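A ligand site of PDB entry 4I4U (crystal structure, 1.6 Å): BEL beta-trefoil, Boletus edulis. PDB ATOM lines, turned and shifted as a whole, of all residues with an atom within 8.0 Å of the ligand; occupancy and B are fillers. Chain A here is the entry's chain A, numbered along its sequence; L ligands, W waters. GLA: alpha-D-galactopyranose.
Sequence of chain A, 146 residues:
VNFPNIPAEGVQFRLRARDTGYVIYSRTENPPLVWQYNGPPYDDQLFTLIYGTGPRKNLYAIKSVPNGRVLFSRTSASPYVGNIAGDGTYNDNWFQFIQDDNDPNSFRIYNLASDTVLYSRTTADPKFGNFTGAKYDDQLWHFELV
The side-chain carboxylate of Asp 138 sits at hydrogen-bond distance from an oxygen (O4) of the ligand (2.5 Å). An oxygen (O6) of the ligand lies within hydrogen-bond range of the side-chain amide nitrogen (NE2) of Gln 139 (2.8 Å). The guanidinium group (NH2) of Arg 121 is in hydrogen-bond range of an oxygen (O4) of the ligand, 3.0 Å away.
O of Asp 138 is in hydrogen-bond range of N of Ser 120 (2.9 Å). NE2 of Gln 139 sits at hydrogen-bond distance from O of Ala 134, 3.0 Å away. OE1 of Gln 139 is in hydrogen-bond range of NE of Arg 108 (2.8 Å). The guanidinium group of Arg 121 is in hydrogen-bond range of the backbone carbonyl oxygen of Ala 124, at 2.9 Å. The guanidinium group (NH1) of Arg 121 sits at hydrogen-bond distance from the backbone carbonyl oxygen (O) of Pro 126 (3.0 Å). N of Arg 121 sits at hydrogen-bond distance from O of Lys 127 (2.9 Å). The side-chain hydroxyl (OH) of Tyr 119 is in hydrogen-bond range of the backbone carbonyl oxygen (O) of Pro 126 (2.7 Å). NH2 of Arg 108 lies within hydrogen-bond range of O of Tyr 136, at 3.2 Å.
Tyr 119 touches the ligand (CB to O6, 3.7 Å). CE1 of Phe 131 touches O5 of the ligand, at 3.6 Å. Tyr 136 touches the ligand (CD1 to O3, 3.7 Å). Hydrophobic or aromatic side chains that line the ligand: Tyr 119, Phe 131 and Tyr 136. Of the 23 residues printed, 6 come within 4 Å of the ligand. The nearest printed residue that does not touch the ligand is Thr 123 (5.2 Å).
Water W2 bridges an oxygen (O1) of the ligand (2.9 Å) and the guanidinium group (NH2) of Arg 121 (3.4 Å). Water W1 bridges O5 of the ligand (3.0 Å) and NH2 of Arg 121 (3.2 Å). Water W3 bridges the side-chain hydroxyl of Thr 123 (2.8 Å) and an oxygen (O3) of the ligand (3.1 Å).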
ATOM      1  N   ARG A 108       1.027  -5.859   6.041  1.00  0.00           N
ATOM      2  CA  ARG A 108       1.564  -4.735   5.296  1.00  0.00           C
ATOM      3  C   ARG A 108       2.865  -5.148   4.628  1.00  0.00           C
ATOM      4  O   ARG A 108       3.617  -5.963   5.177  1.00  0.00           O
ATOM      5  CB  ARG A 108       1.782  -3.525   6.217  1.00  0.00           C
ATOM      6  CG  ARG A 108       0.465  -2.883   6.604  1.00  0.00           C
ATOM      7  CD  ARG A 108       0.556  -1.697   7.552  1.00  0.00           C
ATOM      8  NE  ARG A 108      -0.795  -1.152   7.699  1.00  0.00           N
ATOM      9  CZ  ARG A 108      -1.716  -1.653   8.513  1.00  0.00           C
ATOM     10  NH1 ARG A 108      -1.428  -2.690   9.308  1.00  0.00           N
ATOM     11  NH2 ARG A 108      -2.943  -1.134   8.560  1.00  0.00           N
ATOM     12  N   VAL A 117       5.065   1.685   3.443  1.00  0.00           N
ATOM     13  CA  VAL A 117       4.225   0.535   3.128  1.00  0.00           C
ATOM     14  C   VAL A 117       3.530   0.728   1.779  1.00  0.00           C
ATOM     15  O   VAL A 117       3.301   1.872   1.353  1.00  0.00           O
ATOM     16  CB  VAL A 117       3.185   0.226   4.226  1.00  0.00           C
ATOM     17  CG1 VAL A 117       3.878  -0.028   5.556  1.00  0.00           C
ATOM     18  CG2 VAL A 117       2.154   1.357   4.348  1.00  0.00           C
ATOM     19  N   LEU A 118       3.214  -0.365   1.114  1.00  0.00           N
ATOM     20  CA  LEU A 118       2.458  -0.305  -0.143  1.00  0.00           C
ATOM     21  C   LEU A 118       0.960  -0.207   0.139  1.00  0.00           C
ATOM     22  O   LEU A 118       0.450  -0.790   1.101  1.00  0.00           O
ATOM     23  CB  LEU A 118       2.750  -1.514  -1.032  1.00  0.00           C
ATOM     24  CG  LEU A 118       4.214  -1.757  -1.446  1.00  0.00           C
ATOM     25  CD1 LEU A 118       4.287  -2.967  -2.359  1.00  0.00           C
ATOM     26  CD2 LEU A 118       4.814  -0.538  -2.133  1.00  0.00           C
ATOM     27  N   TYR A 119       0.258   0.533  -0.703  1.00  0.00           N
ATOM     28  CA  TYR A 119      -1.191   0.652  -0.568  1.00  0.00           C
ATOM     29  C   TYR A 119      -1.892   0.503  -1.913  1.00  0.00           C
ATOM     30  O   TYR A 119      -1.320   0.746  -2.982  1.00  0.00           O
ATOM     31  CB  TYR A 119      -1.592   1.990   0.100  1.00  0.00           C
ATOM     32  CG  TYR A 119      -1.360   3.191  -0.779  1.00  0.00           C
ATOM     33  CD1 TYR A 119      -0.182   3.921  -0.683  1.00  0.00           C
ATOM     34  CD2 TYR A 119      -2.306   3.587  -1.721  1.00  0.00           C
ATOM     35  CE1 TYR A 119       0.046   5.014  -1.504  1.00  0.00           C
ATOM     36  CE2 TYR A 119      -2.080   4.661  -2.561  1.00  0.00           C
ATOM     37  CZ  TYR A 119      -0.904   5.389  -2.443  1.00  0.00           C
ATOM     38  OH  TYR A 119      -0.650   6.468  -3.263  1.00  0.00           O
ATOM     39  N   SER A 120      -3.164   0.121  -1.838  1.00  0.00           N
ATOM     40  CA  SER A 120      -4.039  -0.019  -3.000  1.00  0.00           C
ATOM     41  C   SER A 120      -5.394   0.564  -2.639  1.00  0.00           C
ATOM     42  O   SER A 120      -6.039   0.124  -1.696  1.00  0.00           O
ATOM     43  CB  SER A 120      -4.159  -1.492  -3.392  1.00  0.00           C
ATOM     44  OG  SER A 120      -5.274  -1.720  -4.236  1.00  0.00           O
ATOM     45  N   ARG A 121      -5.827   1.582  -3.390  1.00  0.00           N
ATOM     46  CA  ARG A 121      -7.104   2.231  -3.126  1.00  0.00           C
ATOM     47  C   ARG A 121      -7.860   2.571  -4.415  1.00  0.00           C
ATOM     48  O   ARG A 121      -7.316   2.478  -5.504  1.00  0.00           O
ATOM     49  CB  ARG A 121      -6.910   3.489  -2.261  1.00  0.00           C
ATOM     50  CG  ARG A 121      -6.112   4.592  -2.944  1.00  0.00           C
ATOM     51  CD  ARG A 121      -5.708   5.668  -1.949  1.00  0.00           C
ATOM     52  NE  ARG A 121      -5.047   6.758  -2.655  1.00  0.00           N
ATOM     53  CZ  ARG A 121      -4.127   7.555  -2.122  1.00  0.00           C
ATOM     54  NH1 ARG A 121      -3.590   8.504  -2.872  1.00  0.00           N
ATOM     55  NH2 ARG A 121      -3.754   7.410  -0.856  1.00  0.00           N
ATOM     56  N   THR A 122      -9.122   2.962  -4.264  1.00  0.00           N
ATOM     57  CA  THR A 122      -9.960   3.325  -5.405  1.00  0.00           C
ATOM     58  C   THR A 122     -10.263   4.828  -5.400  1.00  0.00           C
ATOM     59  O   THR A 122     -11.025   5.315  -6.232  1.00  0.00           O
ATOM     60  CB  THR A 122     -11.300   2.558  -5.375  1.00  0.00           C
ATOM     61  OG1 THR A 122     -12.011   2.892  -4.179  1.00  0.00           O
ATOM     62  CG2 THR A 122     -11.064   1.060  -5.409  1.00  0.00           C
ATOM     63  N   THR A 123      -9.645   5.547  -4.472  1.00  0.00           N
ATOM     64  CA  THR A 123     -10.023   6.923  -4.177  1.00  0.00           C
ATOM     65  C   THR A 123      -9.133   7.938  -4.913  1.00  0.00           C
ATOM     66  O   THR A 123      -9.308   8.148  -6.105  1.00  0.00           O
ATOM     67  CB  THR A 123     -10.064   7.167  -2.652  1.00  0.00           C
ATOM     68  OG1 THR A 123      -8.836   6.736  -2.062  1.00  0.00           O
ATOM     69  CG2 THR A 123     -11.199   6.385  -2.015  1.00  0.00           C
ATOM     70  N   ALA A 124      -8.180   8.536  -4.203  1.00  0.00           N
ATOM     71  CA  ALA A 124      -7.346   9.590  -4.769  1.00  0.00           C
ATOM     72  C   ALA A 124      -6.179   9.047  -5.563  1.00  0.00           C
ATOM     73  O   ALA A 124      -5.603   8.023  -5.186  1.00  0.00           O
ATOM     74  CB  ALA A 124      -6.852  10.517  -3.674  1.00  0.00           C
ATOM     75  N   PRO A 126      -2.295   9.269  -6.541  1.00  0.00           N
ATOM     76  CA  PRO A 126      -2.079   7.945  -7.162  1.00  0.00           C
ATOM     77  C   PRO A 126      -2.750   6.835  -6.356  1.00  0.00           C
ATOM     78  O   PRO A 126      -2.583   6.776  -5.133  1.00  0.00           O
ATOM     79  CB  PRO A 126      -0.550   7.796  -7.144  1.00  0.00           C
ATOM     80  CG  PRO A 126      -0.107   8.646  -6.005  1.00  0.00           C
ATOM     81  CD  PRO A 126      -1.050   9.814  -5.971  1.00  0.00           C
ATOM     82  N   LYS A 127      -3.489   5.969  -7.040  1.00  0.00           N
ATOM     83  CA  LYS A 127      -4.299   4.947  -6.388  1.00  0.00           C
ATOM     84  C   LYS A 127      -3.475   3.761  -5.884  1.00  0.00           C
ATOM     85  O   LYS A 127      -3.919   3.003  -5.016  1.00  0.00           O
ATOM     86  CB  LYS A 127      -5.428   4.473  -7.324  1.00  0.00           C
ATOM     87  CG  LYS A 127      -6.470   5.543  -7.645  1.00  0.00           C
ATOM     88  CD  LYS A 127      -7.572   4.958  -8.502  1.00  0.00           C
ATOM     89  CE  LYS A 127      -8.781   5.880  -8.583  1.00  0.00           C
ATOM     90  NZ  LYS A 127      -8.620   6.967  -9.582  1.00  0.00           N
ATOM     91  N   GLY A 129       0.713   2.952  -4.620  1.00  0.00           N
ATOM     92  CA  GLY A 129       2.025   3.506  -4.300  1.00  0.00           C
ATOM     93  C   GLY A 129       2.527   3.109  -2.935  1.00  0.00           C
ATOM     94  O   GLY A 129       2.089   2.112  -2.359  1.00  0.00           O
ATOM     95  N   ASN A 130       3.461   3.910  -2.418  1.00  0.00           N
ATOM     96  CA  ASN A 130       3.972   3.712  -1.063  1.00  0.00           C
ATOM     97  C   ASN A 130       3.641   4.899  -0.148  1.00  0.00           C
ATOM     98  O   ASN A 130       3.244   5.973  -0.626  1.00  0.00           O
ATOM     99  CB  ASN A 130       5.458   3.337  -1.053  1.00  0.00           C
ATOM    100  CG  ASN A 130       6.371   4.457  -1.544  1.00  0.00           C
ATOM    101  OD1 ASN A 130       5.935   5.583  -1.828  1.00  0.00           O
ATOM    102  ND2 ASN A 130       7.659   4.153  -1.655  1.00  0.00           N
ATOM    103  N   PHE A 131       3.761   4.690   1.162  1.00  0.00           N
ATOM    104  CA  PHE A 131       3.256   5.643   2.151  1.00  0.00           C
ATOM    105  C   PHE A 131       3.977   5.499   3.488  1.00  0.00           C
ATOM    106  O   PHE A 131       4.204   4.383   3.957  1.00  0.00           O
ATOM    107  CB  PHE A 131       1.741   5.413   2.334  1.00  0.00           C
ATOM    108  CG  PHE A 131       1.082   6.307   3.340  1.00  0.00           C
ATOM    109  CD1 PHE A 131       0.823   7.653   3.036  1.00  0.00           C
ATOM    110  CD2 PHE A 131       0.697   5.812   4.572  1.00  0.00           C
ATOM    111  CE1 PHE A 131       0.197   8.467   3.958  1.00  0.00           C
ATOM    112  CE2 PHE A 131       0.063   6.634   5.508  1.00  0.00           C
ATOM    113  CZ  PHE A 131      -0.182   7.963   5.199  1.00  0.00           C
ATOM    114  N   THR A 132       4.331   6.636   4.083  1.00  0.00           N
ATOM    115  CA  THR A 132       4.850   6.667   5.447  1.00  0.00           C
ATOM    116  C   THR A 132       3.838   7.399   6.315  1.00  0.00           C
ATOM    117  O   THR A 132       3.610   8.601   6.132  1.00  0.00           O
ATOM    118  CB  THR A 132       6.199   7.419   5.543  1.00  0.00           C
ATOM    119  OG1 THR A 132       7.138   6.804   4.656  1.00  0.00           O
ATOM    120  CG2 THR A 132       6.743   7.381   6.954  1.00  0.00           C
ATOM    121  N   GLY A 133       3.231   6.690   7.253  1.00  0.00           N
ATOM    122  CA  GLY A 133       2.243   7.304   8.127  1.00  0.00           C
ATOM    123  C   GLY A 133       1.359   6.312   8.838  1.00  0.00           C
ATOM    124  O   GLY A 133       1.737   5.148   9.006  1.00  0.00           O
ATOM    125  N   ALA A 134       0.182   6.772   9.232  1.00  0.00           N
ATOM    126  CA  ALA A 134      -0.775   5.996  10.017  1.00  0.00           C
ATOM    127  C   ALA A 134      -1.229   4.727   9.304  1.00  0.00           C
ATOM    128  O   ALA A 134      -1.102   4.600   8.084  1.00  0.00           O
ATOM    129  CB  ALA A 134      -1.968   6.855  10.391  1.00  0.00           C
ATOM    130  N   LYS A 135      -1.760   3.798  10.083  1.00  0.00           N
ATOM    131  CA  LYS A 135      -2.249   2.541   9.543  1.00  0.00           C
ATOM    132  C   LYS A 135      -3.652   2.732   8.963  1.00  0.00           C
ATOM    133  O   LYS A 135      -4.548   3.246   9.635  1.00  0.00           O
ATOM    134  CB  LYS A 135      -2.217   1.447  10.608  1.00  0.00           C
ATOM    135  CG  LYS A 135      -0.811   1.157  11.127  1.00  0.00           C
ATOM    136  CD  LYS A 135      -0.729  -0.137  11.924  1.00  0.00           C
ATOM    137  CE  LYS A 135       0.467  -0.152  12.864  1.00  0.00           C
ATOM    138  NZ  LYS A 135       1.718   0.437  12.307  1.00  0.00           N
ATOM    139  N   TYR A 136      -3.782   2.370   7.689  1.00  0.00           N
ATOM    140  CA  TYR A 136      -5.066   2.370   6.996  1.00  0.00           C
ATOM    141  C   TYR A 136      -5.293   0.996   6.394  1.00  0.00           C
ATOM    142  O   TYR A 136      -4.337   0.292   6.060  1.00  0.00           O
ATOM    143  CB  TYR A 136      -5.074   3.412   5.871  1.00  0.00           C
ATOM    144  CG  TYR A 136      -5.047   4.846   6.342  1.00  0.00           C
ATOM    145  CD1 TYR A 136      -6.229   5.516   6.667  1.00  0.00           C
ATOM    146  CD2 TYR A 136      -3.843   5.552   6.430  1.00  0.00           C
ATOM    147  CE1 TYR A 136      -6.211   6.837   7.092  1.00  0.00           C
ATOM    148  CE2 TYR A 136      -3.813   6.867   6.852  1.00  0.00           C
ATOM    149  CZ  TYR A 136      -4.994   7.505   7.187  1.00  0.00           C
ATOM    150  OH  TYR A 136      -4.959   8.821   7.596  1.00  0.00           O
ATOM    151  N   ASP A 137      -6.563   0.627   6.255  1.00  0.00           N
ATOM    152  CA  ASP A 137      -6.942  -0.664   5.718  1.00  0.00           C
ATOM    153  C   ASP A 137      -6.485  -0.914   4.294  1.00  0.00           C
ATOM    154  O   ASP A 137      -6.322  -2.058   3.890  1.00  0.00           O
ATOM    155  CB  ASP A 137      -8.449  -0.835   5.789  1.00  0.00           C
ATOM    156  CG  ASP A 137      -8.949  -1.028   7.193  1.00  0.00           C
ATOM    157  OD1 ASP A 137     -10.184  -0.953   7.398  1.00  0.00           O
ATOM    158  OD2 ASP A 137      -8.119  -1.255   8.097  1.00  0.00           O
ATOM    159  N   ASP A 138      -6.298   0.156   3.521  1.00  0.00           N
ATOM    160  CA  ASP A 138      -5.883   0.008   2.119  1.00  0.00           C
ATOM    161  C   ASP A 138      -4.414  -0.394   1.977  1.00  0.00           C
ATOM    162  O   ASP A 138      -3.912  -0.546   0.853  1.00  0.00           O
ATOM    163  CB  ASP A 138      -6.223   1.261   1.282  1.00  0.00           C
ATOM    164  CG  ASP A 138      -5.442   2.515   1.690  1.00  0.00           C
ATOM    165  OD1 ASP A 138      -4.457   2.458   2.455  1.00  0.00           O
ATOM    166  OD2 ASP A 138      -5.853   3.596   1.207  1.00  0.00           O
ATOM    167  N   GLN A 139      -3.748  -0.582   3.112  1.00  0.00           N
ATOM    168  CA  GLN A 139      -2.360  -1.025   3.162  1.00  0.00           C
ATOM    169  C   GLN A 139      -2.265  -2.533   3.417  1.00  0.00           C
ATOM    170  O   GLN A 139      -1.169  -3.077   3.612  1.00  0.00           O
ATOM    171  CB  GLN A 139      -1.608  -0.272   4.263  1.00  0.00           C
ATOM    172  CG  GLN A 139      -1.592   1.248   4.105  1.00  0.00           C
ATOM    173  CD  GLN A 139      -1.230   1.987   5.385  1.00  0.00           C
ATOM    174  OE1 GLN A 139      -0.908   1.380   6.397  1.00  0.00           O
ATOM    175  NE2 GLN A 139      -1.309   3.312   5.334  1.00  0.00           N
ATOM    176  N   LEU A 140      -3.414  -3.209   3.404  1.00  0.00           N
ATOM    177  CA  LEU A 140      -3.466  -4.626   3.796  1.00  0.00           C
ATOM    178  C   LEU A 140      -3.519  -5.572   2.600  1.00  0.00           C
ATOM    179  O   LEU A 140      -4.310  -5.386   1.683  1.00  0.00           O
ATOM    180  CB  LEU A 140      -4.640  -4.878   4.760  1.00  0.00           C
ATOM    181  CG  LEU A 140      -4.523  -4.131   6.100  1.00  0.00           C
ATOM    182  CD1 LEU A 140      -5.732  -4.408   6.982  1.00  0.00           C
ATOM    183  CD2 LEU A 140      -3.230  -4.471   6.834  1.00  0.00           C
HETATM  184  C1  GLA L   1      -3.791   8.747   1.985  1.00  0.00           C
HETATM  185  C2  GLA L   1      -5.145   8.689   2.732  1.00  0.00           C
HETATM  186  C3  GLA L   1      -5.428   7.371   3.453  1.00  0.00           C
HETATM  187  C4  GLA L   1      -4.667   6.213   2.814  1.00  0.00           C
HETATM  188  C5  GLA L   1      -3.163   6.480   2.858  1.00  0.00           C
HETATM  189  C6  GLA L   1      -2.391   5.371   2.137  1.00  0.00           C
HETATM  190  O1  GLA L   1      -3.127   9.994   2.170  1.00  0.00           O
HETATM  191  O2  GLA L   1      -5.369   9.811   3.620  1.00  0.00           O
HETATM  192  O3  GLA L   1      -6.833   7.110   3.382  1.00  0.00           O
HETATM  193  O4  GLA L   1      -5.100   5.997   1.456  1.00  0.00           O
HETATM  194  O5  GLA L   1      -2.822   7.724   2.235  1.00  0.00           O
HETATM  195  O6  GLA L   1      -2.405   4.187   2.934  1.00  0.00           O
HETATM  196  O   HOH W   1      -0.817   8.309   0.133  1.00  0.00           O
HETATM  197  O   HOH W   2      -4.699  10.659  -0.235  1.00  0.00           O
HETATM  198  O   HOH W   3      -8.403   6.973   0.739  1.00  0.00           O
HETATM  199  O   HOH W   4      -6.098  12.170   1.776  1.00  0.00           O
